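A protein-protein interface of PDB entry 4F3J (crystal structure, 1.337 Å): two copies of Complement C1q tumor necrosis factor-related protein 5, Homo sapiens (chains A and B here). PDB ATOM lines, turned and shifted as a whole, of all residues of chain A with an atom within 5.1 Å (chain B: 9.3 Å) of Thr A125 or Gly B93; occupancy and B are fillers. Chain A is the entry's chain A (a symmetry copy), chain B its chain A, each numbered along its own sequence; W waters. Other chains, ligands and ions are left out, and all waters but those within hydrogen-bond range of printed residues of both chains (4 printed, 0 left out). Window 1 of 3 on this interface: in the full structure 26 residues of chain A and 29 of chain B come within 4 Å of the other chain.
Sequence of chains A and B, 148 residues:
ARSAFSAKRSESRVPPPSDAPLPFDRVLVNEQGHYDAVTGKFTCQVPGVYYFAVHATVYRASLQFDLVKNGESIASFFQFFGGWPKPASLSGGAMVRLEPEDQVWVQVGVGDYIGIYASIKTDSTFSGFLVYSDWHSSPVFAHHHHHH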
ATOM      1  N   SER A   6      -9.187  26.041 -17.386  1.00  0.00           N
ATOM      2  CA  SER A   6      -9.377  25.014 -18.379  1.00  0.00           C
ATOM      3  C   SER A   6     -10.566  25.427 -19.238  1.00  0.00           C
ATOM      4  O   SER A   6     -11.548  25.974 -18.718  1.00  0.00           O
ATOM      5  CB  SER A   6      -9.595  23.655 -17.709  1.00  0.00           C
ATOM      6  OG  SER A   6      -9.654  22.596 -18.667  1.00  0.00           O
ATOM      7  N   ALA A   7     -10.472  25.194 -20.543  1.00  0.00           N
ATOM      8  CA  ALA A   7     -11.517  25.610 -21.481  1.00  0.00           C
ATOM      9  C   ALA A   7     -11.578  24.656 -22.644  1.00  0.00           C
ATOM     10  O   ALA A   7     -10.583  23.965 -22.957  1.00  0.00           O
ATOM     11  CB  ALA A   7     -11.258  27.015 -21.995  1.00  0.00           C
ATOM     12  N   LYS A   8     -12.726  24.604 -23.300  1.00  0.00           N
ATOM     13  CA  LYS A   8     -12.858  23.754 -24.467  1.00  0.00           C
ATOM     14  C   LYS A   8     -13.421  24.485 -25.660  1.00  0.00           C
ATOM     15  O   LYS A   8     -13.979  25.555 -25.522  1.00  0.00           O
ATOM     16  CB  LYS A   8     -13.619  22.484 -24.148  1.00  0.00           C
ATOM     17  CG  LYS A   8     -15.026  22.594 -23.669  1.00  0.00           C
ATOM     18  CD  LYS A   8     -15.382  21.164 -23.215  1.00  0.00           C
ATOM     19  CE  LYS A   8     -16.861  20.898 -23.136  1.00  0.00           C
ATOM     20  NZ  LYS A   8     -17.368  20.958 -21.743  1.00  0.00           N
ATOM     21  N   PHE A  24     -10.573  28.989 -27.043  1.00  0.00           N
ATOM     22  CA  PHE A  24     -11.316  27.869 -26.471  1.00  0.00           C
ATOM     23  C   PHE A  24     -12.411  28.557 -25.682  1.00  0.00           C
ATOM     24  O   PHE A  24     -12.184  29.099 -24.585  1.00  0.00           O
ATOM     25  CB  PHE A  24     -10.428  26.958 -25.604  1.00  0.00           C
ATOM     26  CG  PHE A  24      -9.403  26.181 -26.394  1.00  0.00           C
ATOM     27  CD1 PHE A  24      -9.541  24.806 -26.596  1.00  0.00           C
ATOM     28  CD2 PHE A  24      -8.293  26.829 -26.939  1.00  0.00           C
ATOM     29  CE1 PHE A  24      -8.594  24.089 -27.339  1.00  0.00           C
ATOM     30  CE2 PHE A  24      -7.342  26.123 -27.681  1.00  0.00           C
ATOM     31  CZ  PHE A  24      -7.490  24.754 -27.878  1.00  0.00           C
ATOM     32  N   LEU A  28     -14.348  25.850 -18.538  1.00  0.00           N
ATOM     33  CA  LEU A  28     -14.632  24.870 -17.491  1.00  0.00           C
ATOM     34  C   LEU A  28     -14.343  25.460 -16.124  1.00  0.00           C
ATOM     35  O   LEU A  28     -15.165  25.372 -15.212  1.00  0.00           O
ATOM     36  CB  LEU A  28     -13.816  23.594 -17.687  1.00  0.00           C
ATOM     37  CG  LEU A  28     -14.132  22.817 -18.959  1.00  0.00           C
ATOM     38  CD1 LEU A  28     -13.173  21.657 -19.132  1.00  0.00           C
ATOM     39  CD2 LEU A  28     -15.568  22.319 -18.898  1.00  0.00           C
ATOM     40  N   ALA A  53      -1.369  22.183 -21.083  1.00  0.00           N
ATOM     41  CA  ALA A  53      -1.698  20.963 -21.841  1.00  0.00           C
ATOM     42  C   ALA A  53      -2.867  21.213 -22.753  1.00  0.00           C
ATOM     43  O   ALA A  53      -3.869  21.829 -22.359  1.00  0.00           O
ATOM     44  CB  ALA A  53      -1.995  19.776 -20.885  1.00  0.00           C
ATOM     45  N   VAL A  54      -2.776  20.659 -23.964  1.00  0.00           N
ATOM     46  CA  VAL A  54      -3.847  20.648 -24.961  1.00  0.00           C
ATOM     47  C   VAL A  54      -4.162  19.197 -25.254  1.00  0.00           C
ATOM     48  O   VAL A  54      -3.260  18.382 -25.463  1.00  0.00           O
ATOM     49  CB  VAL A  54      -3.424  21.380 -26.247  1.00  0.00           C
ATOM     50  CG1 VAL A  54      -4.489  21.247 -27.321  1.00  0.00           C
ATOM     51  CG2 VAL A  54      -3.179  22.869 -25.926  1.00  0.00           C
ATOM     52  N   HIS A  55      -5.449  18.867 -25.214  1.00  0.00           N
ATOM     53  CA  HIS A  55      -5.928  17.550 -25.603  1.00  0.00           C
ATOM     54  C   HIS A  55      -6.944  17.775 -26.705  1.00  0.00           C
ATOM     55  O   HIS A  55      -8.075  18.192 -26.416  1.00  0.00           O
ATOM     56  CB  HIS A  55      -6.523  16.801 -24.384  1.00  0.00           C
ATOM     57  CG  HIS A  55      -5.553  16.623 -23.260  1.00  0.00           C
ATOM     58  ND1 HIS A  55      -4.589  15.640 -23.256  1.00  0.00           N
ATOM     59  CD2 HIS A  55      -5.381  17.314 -22.108  1.00  0.00           C
ATOM     60  CE1 HIS A  55      -3.870  15.728 -22.160  1.00  0.00           C
ATOM     61  NE2 HIS A  55      -4.335  16.737 -21.431  1.00  0.00           N
ATOM     62  N   ALA A  56      -6.536  17.539 -27.951  1.00  0.00           N
ATOM     63  CA  ALA A  56      -7.348  17.885 -29.118  1.00  0.00           C
ATOM     64  C   ALA A  56      -7.912  16.692 -29.872  1.00  0.00           C
ATOM     65  O   ALA A  56      -7.264  15.645 -29.975  1.00  0.00           O
ATOM     66  CB  ALA A  56      -6.523  18.717 -30.099  1.00  0.00           C
ATOM     67  N   ASP A 123     -14.164  16.501 -27.791  1.00  0.00           N
ATOM     68  CA  ASP A 123     -13.776  17.846 -27.389  1.00  0.00           C
ATOM     69  C   ASP A 123     -12.313  18.131 -27.698  1.00  0.00           C
ATOM     70  O   ASP A 123     -11.505  17.223 -27.915  1.00  0.00           O
ATOM     71  CB  ASP A 123     -13.968  18.021 -25.875  1.00  0.00           C
ATOM     72  CG  ASP A 123     -15.410  18.230 -25.491  1.00  0.00           C
ATOM     73  OD1 ASP A 123     -16.049  19.119 -26.087  1.00  0.00           O
ATOM     74  OD2 ASP A 123     -15.897  17.514 -24.585  1.00  0.00           O
ATOM     75  N   SER A 124     -11.963  19.409 -27.667  1.00  0.00           N
ATOM     76  CA  SER A 124     -10.563  19.813 -27.648  1.00  0.00           C
ATOM     77  C   SER A 124     -10.421  20.766 -26.460  1.00  0.00           C
ATOM     78  O   SER A 124     -11.159  21.749 -26.377  1.00  0.00           O
ATOM     79  CB  SER A 124     -10.160  20.496 -28.959  1.00  0.00           C
ATOM     80  OG  SER A 124     -10.212  19.594 -30.062  1.00  0.00           O
ATOM     81  N   THR A 125      -9.532  20.454 -25.510  1.00  0.00           N
ATOM     82  CA  THR A 125      -9.352  21.263 -24.293  1.00  0.00           C
ATOM     83  C   THR A 125      -7.976  21.909 -24.237  1.00  0.00           C
ATOM     84  O   THR A 125      -6.980  21.372 -24.746  1.00  0.00           O
ATOM     85  CB  THR A 125      -9.557  20.415 -23.007  1.00  0.00           C
ATOM     86  OG1 THR A 125      -8.494  19.458 -22.878  1.00  0.00           O
ATOM     87  CG2 THR A 125     -10.910  19.693 -23.026  1.00  0.00           C
ATOM     88  N   PHE A 126      -7.916  23.047 -23.544  1.00  0.00           N
ATOM     89  CA  PHE A 126      -6.692  23.802 -23.263  1.00  0.00           C
ATOM     90  C   PHE A 126      -6.745  24.091 -21.775  1.00  0.00           C
ATOM     91  O   PHE A 126      -7.749  24.639 -21.287  1.00  0.00           O
ATOM     92  CB  PHE A 126      -6.722  25.104 -24.076  1.00  0.00           C
ATOM     93  CG  PHE A 126      -5.536  26.023 -23.880  1.00  0.00           C
ATOM     94  CD1 PHE A 126      -4.275  25.540 -23.548  1.00  0.00           C
ATOM     95  CD2 PHE A 126      -5.697  27.393 -24.086  1.00  0.00           C
ATOM     96  CE1 PHE A 126      -3.179  26.423 -23.389  1.00  0.00           C
ATOM     97  CE2 PHE A 126      -4.639  28.287 -23.923  1.00  0.00           C
ATOM     98  CZ  PHE A 126      -3.381  27.805 -23.566  1.00  0.00           C
ATOM     99  N   SER A 127      -5.694  23.714 -21.038  1.00  0.00           N
ATOM    100  CA  SER A 127      -5.610  23.917 -19.588  1.00  0.00           C
ATOM    101  C   SER A 127      -4.246  24.437 -19.235  1.00  0.00           C
ATOM    102  O   SER A 127      -3.251  24.141 -19.897  1.00  0.00           O
ATOM    103  CB  SER A 127      -5.777  22.575 -18.869  1.00  0.00           C
ATOM    104  OG  SER A 127      -6.991  21.928 -19.217  1.00  0.00           O
ATOM    105  N   TYR B  50      -8.806  21.058  -9.582  1.00  0.00           N
ATOM    106  CA  TYR B  50      -8.109  19.790  -9.837  1.00  0.00           C
ATOM    107  C   TYR B  50      -7.769  19.640 -11.312  1.00  0.00           C
ATOM    108  O   TYR B  50      -8.547  20.097 -12.167  1.00  0.00           O
ATOM    109  CB  TYR B  50      -9.009  18.595  -9.449  1.00  0.00           C
ATOM    110  CG  TYR B  50      -9.177  18.451  -7.942  1.00  0.00           C
ATOM    111  CD1 TYR B  50      -8.519  17.431  -7.245  1.00  0.00           C
ATOM    112  CD2 TYR B  50      -9.968  19.342  -7.199  1.00  0.00           C
ATOM    113  CE1 TYR B  50      -8.637  17.304  -5.842  1.00  0.00           C
ATOM    114  CE2 TYR B  50     -10.082  19.213  -5.800  1.00  0.00           C
ATOM    115  CZ  TYR B  50      -9.416  18.183  -5.155  1.00  0.00           C
ATOM    116  OH  TYR B  50      -9.505  18.037  -3.787  1.00  0.00           O
ATOM    117  N   TYR B  51      -6.635  18.993 -11.615  1.00  0.00           N
ATOM    118  CA  TYR B  51      -6.370  18.533 -12.980  1.00  0.00           C
ATOM    119  C   TYR B  51      -6.547  17.018 -13.042  1.00  0.00           C
ATOM    120  O   TYR B  51      -6.103  16.312 -12.135  1.00  0.00           O
ATOM    121  CB  TYR B  51      -4.941  18.917 -13.372  1.00  0.00           C
ATOM    122  CG  TYR B  51      -4.553  18.486 -14.784  1.00  0.00           C
ATOM    123  CD1 TYR B  51      -5.221  19.002 -15.911  1.00  0.00           C
ATOM    124  CD2 TYR B  51      -3.502  17.602 -15.006  1.00  0.00           C
ATOM    125  CE1 TYR B  51      -4.858  18.629 -17.210  1.00  0.00           C
ATOM    126  CE2 TYR B  51      -3.135  17.225 -16.311  1.00  0.00           C
ATOM    127  CZ  TYR B  51      -3.809  17.774 -17.385  1.00  0.00           C
ATOM    128  OH  TYR B  51      -3.499  17.439 -18.697  1.00  0.00           O
ATOM    129  N   PHE B  52      -7.206  16.519 -14.091  1.00  0.00           N
ATOM    130  CA  PHE B  52      -7.360  15.087 -14.345  1.00  0.00           C
ATOM    131  C   PHE B  52      -6.838  14.804 -15.735  1.00  0.00           C
ATOM    132  O   PHE B  52      -7.081  15.573 -16.657  1.00  0.00           O
ATOM    133  CB  PHE B  52      -8.838  14.684 -14.269  1.00  0.00           C
ATOM    134  CG  PHE B  52      -9.413  14.763 -12.865  1.00  0.00           C
ATOM    135  CD1 PHE B  52      -9.317  13.664 -11.991  1.00  0.00           C
ATOM    136  CD2 PHE B  52     -10.073  15.907 -12.416  1.00  0.00           C
ATOM    137  CE1 PHE B  52      -9.841  13.724 -10.698  1.00  0.00           C
ATOM    138  CE2 PHE B  52     -10.576  15.978 -11.116  1.00  0.00           C
ATOM    139  CZ  PHE B  52     -10.469  14.887 -10.265  1.00  0.00           C
ATOM    140  N   ALA B  53      -6.157  13.681 -15.876  1.00  0.00           N
ATOM    141  CA  ALA B  53      -5.618  13.240 -17.174  1.00  0.00           C
ATOM    142  C   ALA B  53      -5.752  11.749 -17.318  1.00  0.00           C
ATOM    143  O   ALA B  53      -5.463  10.985 -16.385  1.00  0.00           O
ATOM    144  CB  ALA B  53      -4.136  13.674 -17.340  1.00  0.00           C
ATOM    145  N   VAL B  54      -6.118  11.323 -18.528  1.00  0.00           N
ATOM    146  CA  VAL B  54      -6.172   9.919 -18.939  1.00  0.00           C
ATOM    147  C   VAL B  54      -5.219   9.762 -20.105  1.00  0.00           C
ATOM    148  O   VAL B  54      -5.222  10.569 -21.038  1.00  0.00           O
ATOM    149  CB  VAL B  54      -7.597   9.508 -19.347  1.00  0.00           C
ATOM    150  CG1 VAL B  54      -7.617   8.094 -19.897  1.00  0.00           C
ATOM    151  CG2 VAL B  54      -8.526   9.611 -18.119  1.00  0.00           C
ATOM    152  N   HIS B  55      -4.364   8.748 -20.019  1.00  0.00           N
ATOM    153  CA  HIS B  55      -3.478   8.381 -21.112  1.00  0.00           C
ATOM    154  C   HIS B  55      -3.775   6.930 -21.434  1.00  0.00           C
ATOM    155  O   HIS B  55      -3.353   6.039 -20.682  1.00  0.00           O
ATOM    156  CB  HIS B  55      -1.997   8.615 -20.720  1.00  0.00           C
ATOM    157  CG  HIS B  55      -1.696  10.030 -20.341  1.00  0.00           C
ATOM    158  ND1 HIS B  55      -1.494  11.025 -21.271  1.00  0.00           N
ATOM    159  CD2 HIS B  55      -1.581  10.627 -19.131  1.00  0.00           C
ATOM    160  CE1 HIS B  55      -1.267  12.166 -20.659  1.00  0.00           C
ATOM    161  NE2 HIS B  55      -1.305  11.954 -19.348  1.00  0.00           N
ATOM    162  N   PHE B  65     -14.073   8.040 -24.550  1.00  0.00           N
ATOM    163  CA  PHE B  65     -14.330   8.164 -23.111  1.00  0.00           C
ATOM    164  C   PHE B  65     -14.669   9.586 -22.702  1.00  0.00           C
ATOM    165  O   PHE B  65     -14.244  10.561 -23.358  1.00  0.00           O
ATOM    166  CB  PHE B  65     -13.178   7.599 -22.235  1.00  0.00           C
ATOM    167  CG  PHE B  65     -11.897   8.401 -22.284  1.00  0.00           C
ATOM    168  CD1 PHE B  65     -11.716   9.519 -21.469  1.00  0.00           C
ATOM    169  CD2 PHE B  65     -10.849   7.996 -23.084  1.00  0.00           C
ATOM    170  CE1 PHE B  65     -10.546  10.244 -21.519  1.00  0.00           C
ATOM    171  CE2 PHE B  65      -9.677   8.720 -23.142  1.00  0.00           C
ATOM    172  CZ  PHE B  65      -9.519   9.839 -22.338  1.00  0.00           C
ATOM    173  N   ASP B  66     -15.443   9.684 -21.623  1.00  0.00           N
ATOM    174  CA  ASP B  66     -15.748  10.946 -20.976  1.00  0.00           C
ATOM    175  C   ASP B  66     -15.036  11.032 -19.629  1.00  0.00           C
ATOM    176  O   ASP B  66     -14.927  10.034 -18.909  1.00  0.00           O
ATOM    177  CB  ASP B  66     -17.253  11.053 -20.700  1.00  0.00           C
ATOM    178  CG  ASP B  66     -18.091  11.088 -21.959  1.00  0.00           C
ATOM    179  OD1 ASP B  66     -17.602  11.576 -22.994  1.00  0.00           O
ATOM    180  OD2 ASP B  66     -19.257  10.634 -21.912  1.00  0.00           O
ATOM    181  N   LEU B  67     -14.560  12.226 -19.291  1.00  0.00           N
ATOM    182  CA  LEU B  67     -14.238  12.548 -17.904  1.00  0.00           C
ATOM    183  C   LEU B  67     -15.529  13.068 -17.311  1.00  0.00           C
ATOM    184  O   LEU B  67     -16.158  13.970 -17.894  1.00  0.00           O
ATOM    185  CB  LEU B  67     -13.152  13.615 -17.838  1.00  0.00           C
ATOM    186  CG  LEU B  67     -11.725  13.107 -18.058  1.00  0.00           C
ATOM    187  CD1 LEU B  67     -10.787  14.278 -18.291  1.00  0.00           C
ATOM    188  CD2 LEU B  67     -11.284  12.353 -16.792  1.00  0.00           C
ATOM    189  N   ILE B  74     -17.628  16.192 -18.198  1.00  0.00           N
ATOM    190  CA  ILE B  74     -16.794  17.390 -18.211  1.00  0.00           C
ATOM    191  C   ILE B  74     -16.235  17.621 -19.619  1.00  0.00           C
ATOM    192  O   ILE B  74     -16.273  18.723 -20.171  1.00  0.00           O
ATOM    193  CB  ILE B  74     -15.553  17.218 -17.246  1.00  0.00           C
ATOM    194  CG1 ILE B  74     -15.973  16.967 -15.796  1.00  0.00           C
ATOM    195  CG2 ILE B  74     -14.618  18.413 -17.341  1.00  0.00           C
ATOM    196  CD1 ILE B  74     -14.844  16.394 -14.928  1.00  0.00           C
ATOM    197  N   ALA B  75     -15.693  16.555 -20.190  1.00  0.00           N
ATOM    198  CA  ALA B  75     -15.064  16.590 -21.512  1.00  0.00           C
ATOM    199  C   ALA B  75     -15.029  15.175 -22.036  1.00  0.00           C
ATOM    200  O   ALA B  75     -14.936  14.217 -21.267  1.00  0.00           O
ATOM    201  CB  ALA B  75     -13.635  17.171 -21.432  1.00  0.00           C
ATOM    202  N   SER B  76     -15.071  15.073 -23.359  1.00  0.00           N
ATOM    203  CA  SER B  76     -15.188  13.821 -24.088  1.00  0.00           C
ATOM    204  C   SER B  76     -14.051  13.689 -25.098  1.00  0.00           C
ATOM    205  O   SER B  76     -13.653  14.686 -25.719  1.00  0.00           O
ATOM    206  CB  SER B  76     -16.515  13.796 -24.849  1.00  0.00           C
ATOM    207  OG  SER B  76     -17.625  13.951 -23.967  1.00  0.00           O
ATOM    208  N   PHE B  77     -13.531  12.467 -25.273  1.00  0.00           N
ATOM    209  CA  PHE B  77     -12.386  12.230 -26.142  1.00  0.00           C
ATOM    210  C   PHE B  77     -12.609  10.988 -27.000  1.00  0.00           C
ATOM    211  O   PHE B  77     -13.396  10.110 -26.648  1.00  0.00           O
ATOM    212  CB  PHE B  77     -11.093  12.158 -25.312  1.00  0.00           C
ATOM    213  CG  PHE B  77     -10.867  13.399 -24.519  1.00  0.00           C
ATOM    214  CD1 PHE B  77     -10.267  14.509 -25.117  1.00  0.00           C
ATOM    215  CD2 PHE B  77     -11.327  13.505 -23.203  1.00  0.00           C
ATOM    216  CE1 PHE B  77     -10.083  15.681 -24.415  1.00  0.00           C
ATOM    217  CE2 PHE B  77     -11.139  14.675 -22.488  1.00  0.00           C
ATOM    218  CZ  PHE B  77     -10.512  15.770 -23.101  1.00  0.00           C
ATOM    219  N   LEU B  90      -4.667   7.483 -27.008  1.00  0.00           N
ATOM    220  CA  LEU B  90      -5.633   8.564 -26.799  1.00  0.00           C
ATOM    221  C   LEU B  90      -5.409   9.165 -25.434  1.00  0.00           C
ATOM    222  O   LEU B  90      -5.482   8.458 -24.431  1.00  0.00           O
ATOM    223  CB  LEU B  90      -7.068   8.004 -26.838  1.00  0.00           C
ATOM    224  CG  LEU B  90      -8.200   8.982 -26.487  1.00  0.00           C
ATOM    225  CD1 LEU B  90      -8.179  10.207 -27.374  1.00  0.00           C
ATOM    226  CD2 LEU B  90      -9.538   8.276 -26.549  1.00  0.00           C
ATOM    227  N   SER B  91      -5.186  10.470 -25.365  1.00  0.00           N
ATOM    228  CA  SER B  91      -5.107  11.139 -24.077  1.00  0.00           C
ATOM    229  C   SER B  91      -6.182  12.198 -23.996  1.00  0.00           C
ATOM    230  O   SER B  91      -6.590  12.795 -24.996  1.00  0.00           O
ATOM    231  CB  SER B  91      -3.741  11.777 -23.909  1.00  0.00           C
ATOM    232  OG  SER B  91      -2.737  10.785 -23.766  1.00  0.00           O
ATOM    233  N   GLY B  92      -6.636  12.450 -22.782  1.00  0.00           N
ATOM    234  CA  GLY B  92      -7.618  13.490 -22.520  1.00  0.00           C
ATOM    235  C   GLY B  92      -7.350  14.093 -21.160  1.00  0.00           C
ATOM    236  O   GLY B  92      -6.758  13.462 -20.290  1.00  0.00           O
ATOM    237  N   GLY B  93      -7.788  15.323 -20.955  1.00  0.00           N
ATOM    238  CA  GLY B  93      -7.527  15.965 -19.691  1.00  0.00           C
ATOM    239  C   GLY B  93      -8.333  17.235 -19.597  1.00  0.00           C
ATOM    240  O   GLY B  93      -8.770  17.774 -20.633  1.00  0.00           O
ATOM    241  N   ALA B  94      -8.513  17.730 -18.376  1.00  0.00           N
ATOM    242  CA  ALA B  94      -9.262  18.955 -18.123  1.00  0.00           C
ATOM    243  C   ALA B  94      -9.064  19.344 -16.667  1.00  0.00           C
ATOM    244  O   ALA B  94      -8.622  18.520 -15.848  1.00  0.00           O
ATOM    245  CB  ALA B  94     -10.776  18.772 -18.404  1.00  0.00           C
ATOM    246  N   MET B  95      -9.395  20.593 -16.324  1.00  0.00           N
ATOM    247  CA  MET B  95      -9.491  20.996 -14.913  1.00  0.00           C
ATOM    248  C   MET B  95     -10.947  21.214 -14.553  1.00  0.00           C
ATOM    249  O   MET B  95     -11.778  21.553 -15.405  1.00  0.00           O
ATOM    250  CB  MET B  95      -8.687  22.274 -14.596  1.00  0.00           C
ATOM    251  CG  MET B  95      -7.215  22.237 -15.078  1.00  0.00           C
ATOM    252  SD  MET B  95      -6.276  23.606 -14.450  1.00  0.00           S
ATOM    253  CE  MET B  95      -5.833  22.934 -12.862  1.00  0.00           C
ATOM    254  N   VAL B  96     -11.246  21.073 -13.263  1.00  0.00           N
ATOM    255  CA  VAL B  96     -12.588  21.230 -12.775  1.00  0.00           C
ATOM    256  C   VAL B  96     -12.495  21.666 -11.323  1.00  0.00           C
ATOM    257  O   VAL B  96     -11.548  21.324 -10.601  1.00  0.00           O
ATOM    258  CB  VAL B  96     -13.396  19.914 -12.934  1.00  0.00           C
ATOM    259  CG1 VAL B  96     -12.811  18.788 -12.129  1.00  0.00           C
ATOM    260  CG2 VAL B  96     -14.863  20.109 -12.644  1.00  0.00           C
ATOM    261  N   VAL B 106     -13.840   8.124 -15.074  1.00  0.00           N
ATOM    262  CA  VAL B 106     -13.764   7.951 -16.518  1.00  0.00           C
ATOM    263  C   VAL B 106     -14.889   7.010 -16.926  1.00  0.00           C
ATOM    264  O   VAL B 106     -15.150   6.018 -16.239  1.00  0.00           O
ATOM    265  CB  VAL B 106     -12.411   7.322 -16.912  1.00  0.00           C
ATOM    266  CG1 VAL B 106     -12.316   7.109 -18.427  1.00  0.00           C
ATOM    267  CG2 VAL B 106     -11.254   8.172 -16.385  1.00  0.00           C
ATOM    268  N   THR B 125      -3.656   4.853 -18.121  1.00  0.00           N
ATOM    269  CA  THR B 125      -3.586   5.468 -16.785  1.00  0.00           C
ATOM    270  C   THR B 125      -4.640   6.550 -16.601  1.00  0.00           C
ATOM    271  O   THR B 125      -5.045   7.237 -17.551  1.00  0.00           O
ATOM    272  CB  THR B 125      -2.186   6.084 -16.512  1.00  0.00           C
ATOM    273  OG1 THR B 125      -1.977   7.221 -17.364  1.00  0.00           O
ATOM    274  CG2 THR B 125      -1.072   5.054 -16.732  1.00  0.00           C
ATOM    275  N   PHE B 126      -5.033   6.744 -15.341  1.00  0.00           N
ATOM    276  CA  PHE B 126      -5.958   7.789 -14.896  1.00  0.00           C
ATOM    277  C   PHE B 126      -5.276   8.433 -13.705  1.00  0.00           C
ATOM    278  O   PHE B 126      -4.887   7.726 -12.759  1.00  0.00           O
ATOM    279  CB  PHE B 126      -7.281   7.127 -14.480  1.00  0.00           C
ATOM    280  CG  PHE B 126      -8.346   8.070 -13.963  1.00  0.00           C
ATOM    281  CD1 PHE B 126      -8.432   9.392 -14.387  1.00  0.00           C
ATOM    282  CD2 PHE B 126      -9.304   7.588 -13.071  1.00  0.00           C
ATOM    283  CE1 PHE B 126      -9.452  10.244 -13.900  1.00  0.00           C
ATOM    284  CE2 PHE B 126     -10.312   8.409 -12.565  1.00  0.00           C
ATOM    285  CZ  PHE B 126     -10.382   9.739 -12.970  1.00  0.00           C
ATOM    286  N   SER B 127      -5.101   9.759 -13.740  1.00  0.00           N
ATOM    287  CA  SER B 127      -4.448  10.516 -12.667  1.00  0.00           C
ATOM    288  C   SER B 127      -5.242  11.758 -12.378  1.00  0.00           C
ATOM    289  O   SER B 127      -5.895  12.326 -13.253  1.00  0.00           O
ATOM    290  CB  SER B 127      -3.061  10.970 -13.128  1.00  0.00           C
ATOM    291  OG  SER B 127      -2.250   9.880 -13.541  1.00  0.00           O
HETATM  292  O   HOH W   1     -18.366  16.539 -22.841  1.00  0.00           O
HETATM  293  O   HOH W   2     -18.612  16.602 -25.976  1.00  0.00           O
HETATM  294  O   HOH W   3      -7.465  14.065 -27.340  1.00  0.00           O
HETATM  295  O   HOH W   4     -18.363  20.538 -19.304  1.00  0.00           O
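Of the 14 printed residues of chain A, 8 touch a printed residue of chain B. Printed residues of chain A that touch a printed residue of chain B: Ser A6, Lys A8, Leu A28, Ala A53, His A55, Asp A123, Thr A125 and Ser A127.
N of Phe B52 is in hydrogen-bond range of O of Ala B94 (3.0 Å). A ring nitrogen (ND1) of His B55 lies within hydrogen-bond range of the side-chain hydroxyl of Ser B91 (2.8 Å). The backbone carbonyl oxygen (O) of Phe B65 lies within hydrogen-bond range of the backbone NH (N) of Phe B77 (2.8 Å). The backbone NH (N) of Ile B74 sits at hydrogen-bond distance from the backbone carbonyl oxygen (O) of Leu B67 (2.7 Å). O of Ser A6 sits at hydrogen-bond distance from N of Leu A28 (2.8 Å). The backbone carbonyl oxygen (O) of Ala A53 sits at hydrogen-bond distance from the backbone NH (N) of Ser A127, at 2.9 Å.
Leu A28 touches Ala B94. Leu A28 touches Met B95 (CB to O, 3.7 Å). Tyr B51 touches Ala A53. His A55 touches Phe B77 (CB to CE1, 3.7 Å). Ser B91 touches His A55. Gly B92 touches His A55 (C to CG, 3.7 Å). His A55 touches Gly B93 (CD2 to N, 3.3 Å). CA of Ala B75 touches OD2 of Asp A123, at 3.3 Å. Ser A127 touches Ala B94 (OG to CA, 3.9 Å). Ser A127 touches Met B95 (OG to N, 3.99 Å).
Water W4 lies within hydrogen-bond range of the side-chain amino group (NZ) of Lys A8 (2.7 Å) and the backbone carbonyl oxygen (O) of Ile B74 (2.9 Å). Water W3 lies within hydrogen-bond range of O of Ser B91 (2.8 Å) and O of Ala A56 (3.1 Å). Water W1 bridges the side-chain hydroxyl (OG) of Ser B76 (2.9 Å) and the side-chain carboxylate (OD2) of Asp A123 (3.2 Å). Water W2 bridges the side-chain carboxylate (OD2) of Asp A123 and the side-chain hydroxyl (OG) of Ser B76.
Positions printed for both chains: 53, 54, 55, 125, 126 and 127. Of the 18 pairs that touch across the chains among the printed residues, none has its exchanged pair printed and touching as well.
Of chain B, only Phe B77 (3.9 Å) and Gly B93 (2.8 Å) come within 4 Å of Thr A125. Gly B93 touches just these residues of chain A: His A55 (3.3 Å) and Thr A125 (2.8 Å). No residue of chain B comes within 4 Å of Val A54. His A55 touches five residues of chain B. No residue of chain B comes within 4 Å of Ser A124. Of the printed residues of chain A, Ser B76 touches Asp A123. Printed residues of chain A within 4 Å of Ile B74: Lys A8 and Leu A28. Printed residues of chain B within 4 Å of Ser A127: Ala B94 and Met B95. His B55 touches none of the printed residues of chain A. Leu B67 touches none of the printed residues of chain A. The nearest printed residue of chain B that does not touch Lys A8 is Ala B75 (4.7 Å).
OH of Tyr B51 is in hydrogen-bond range of NE2 of His A55, 2.9 Å away. The side-chain amino group (NZ) of Lys A8 sits at hydrogen-bond distance from the backbone carbonyl oxygen (O) of Ile B74 (2.9 Å). O of Ser B76 sits at hydrogen-bond distance from N of Asp A123, 2.8 Å away. The side-chain hydroxyl (OG1) of Thr A125 is in hydrogen-bond range of the backbone carbonyl oxygen (O) of Gly B93 (2.8 Å). The backbone NH (N) of Met B95 is in hydrogen-bond range of the side-chain hydroxyl (OG) of Ser A6, 3.1 Å away.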
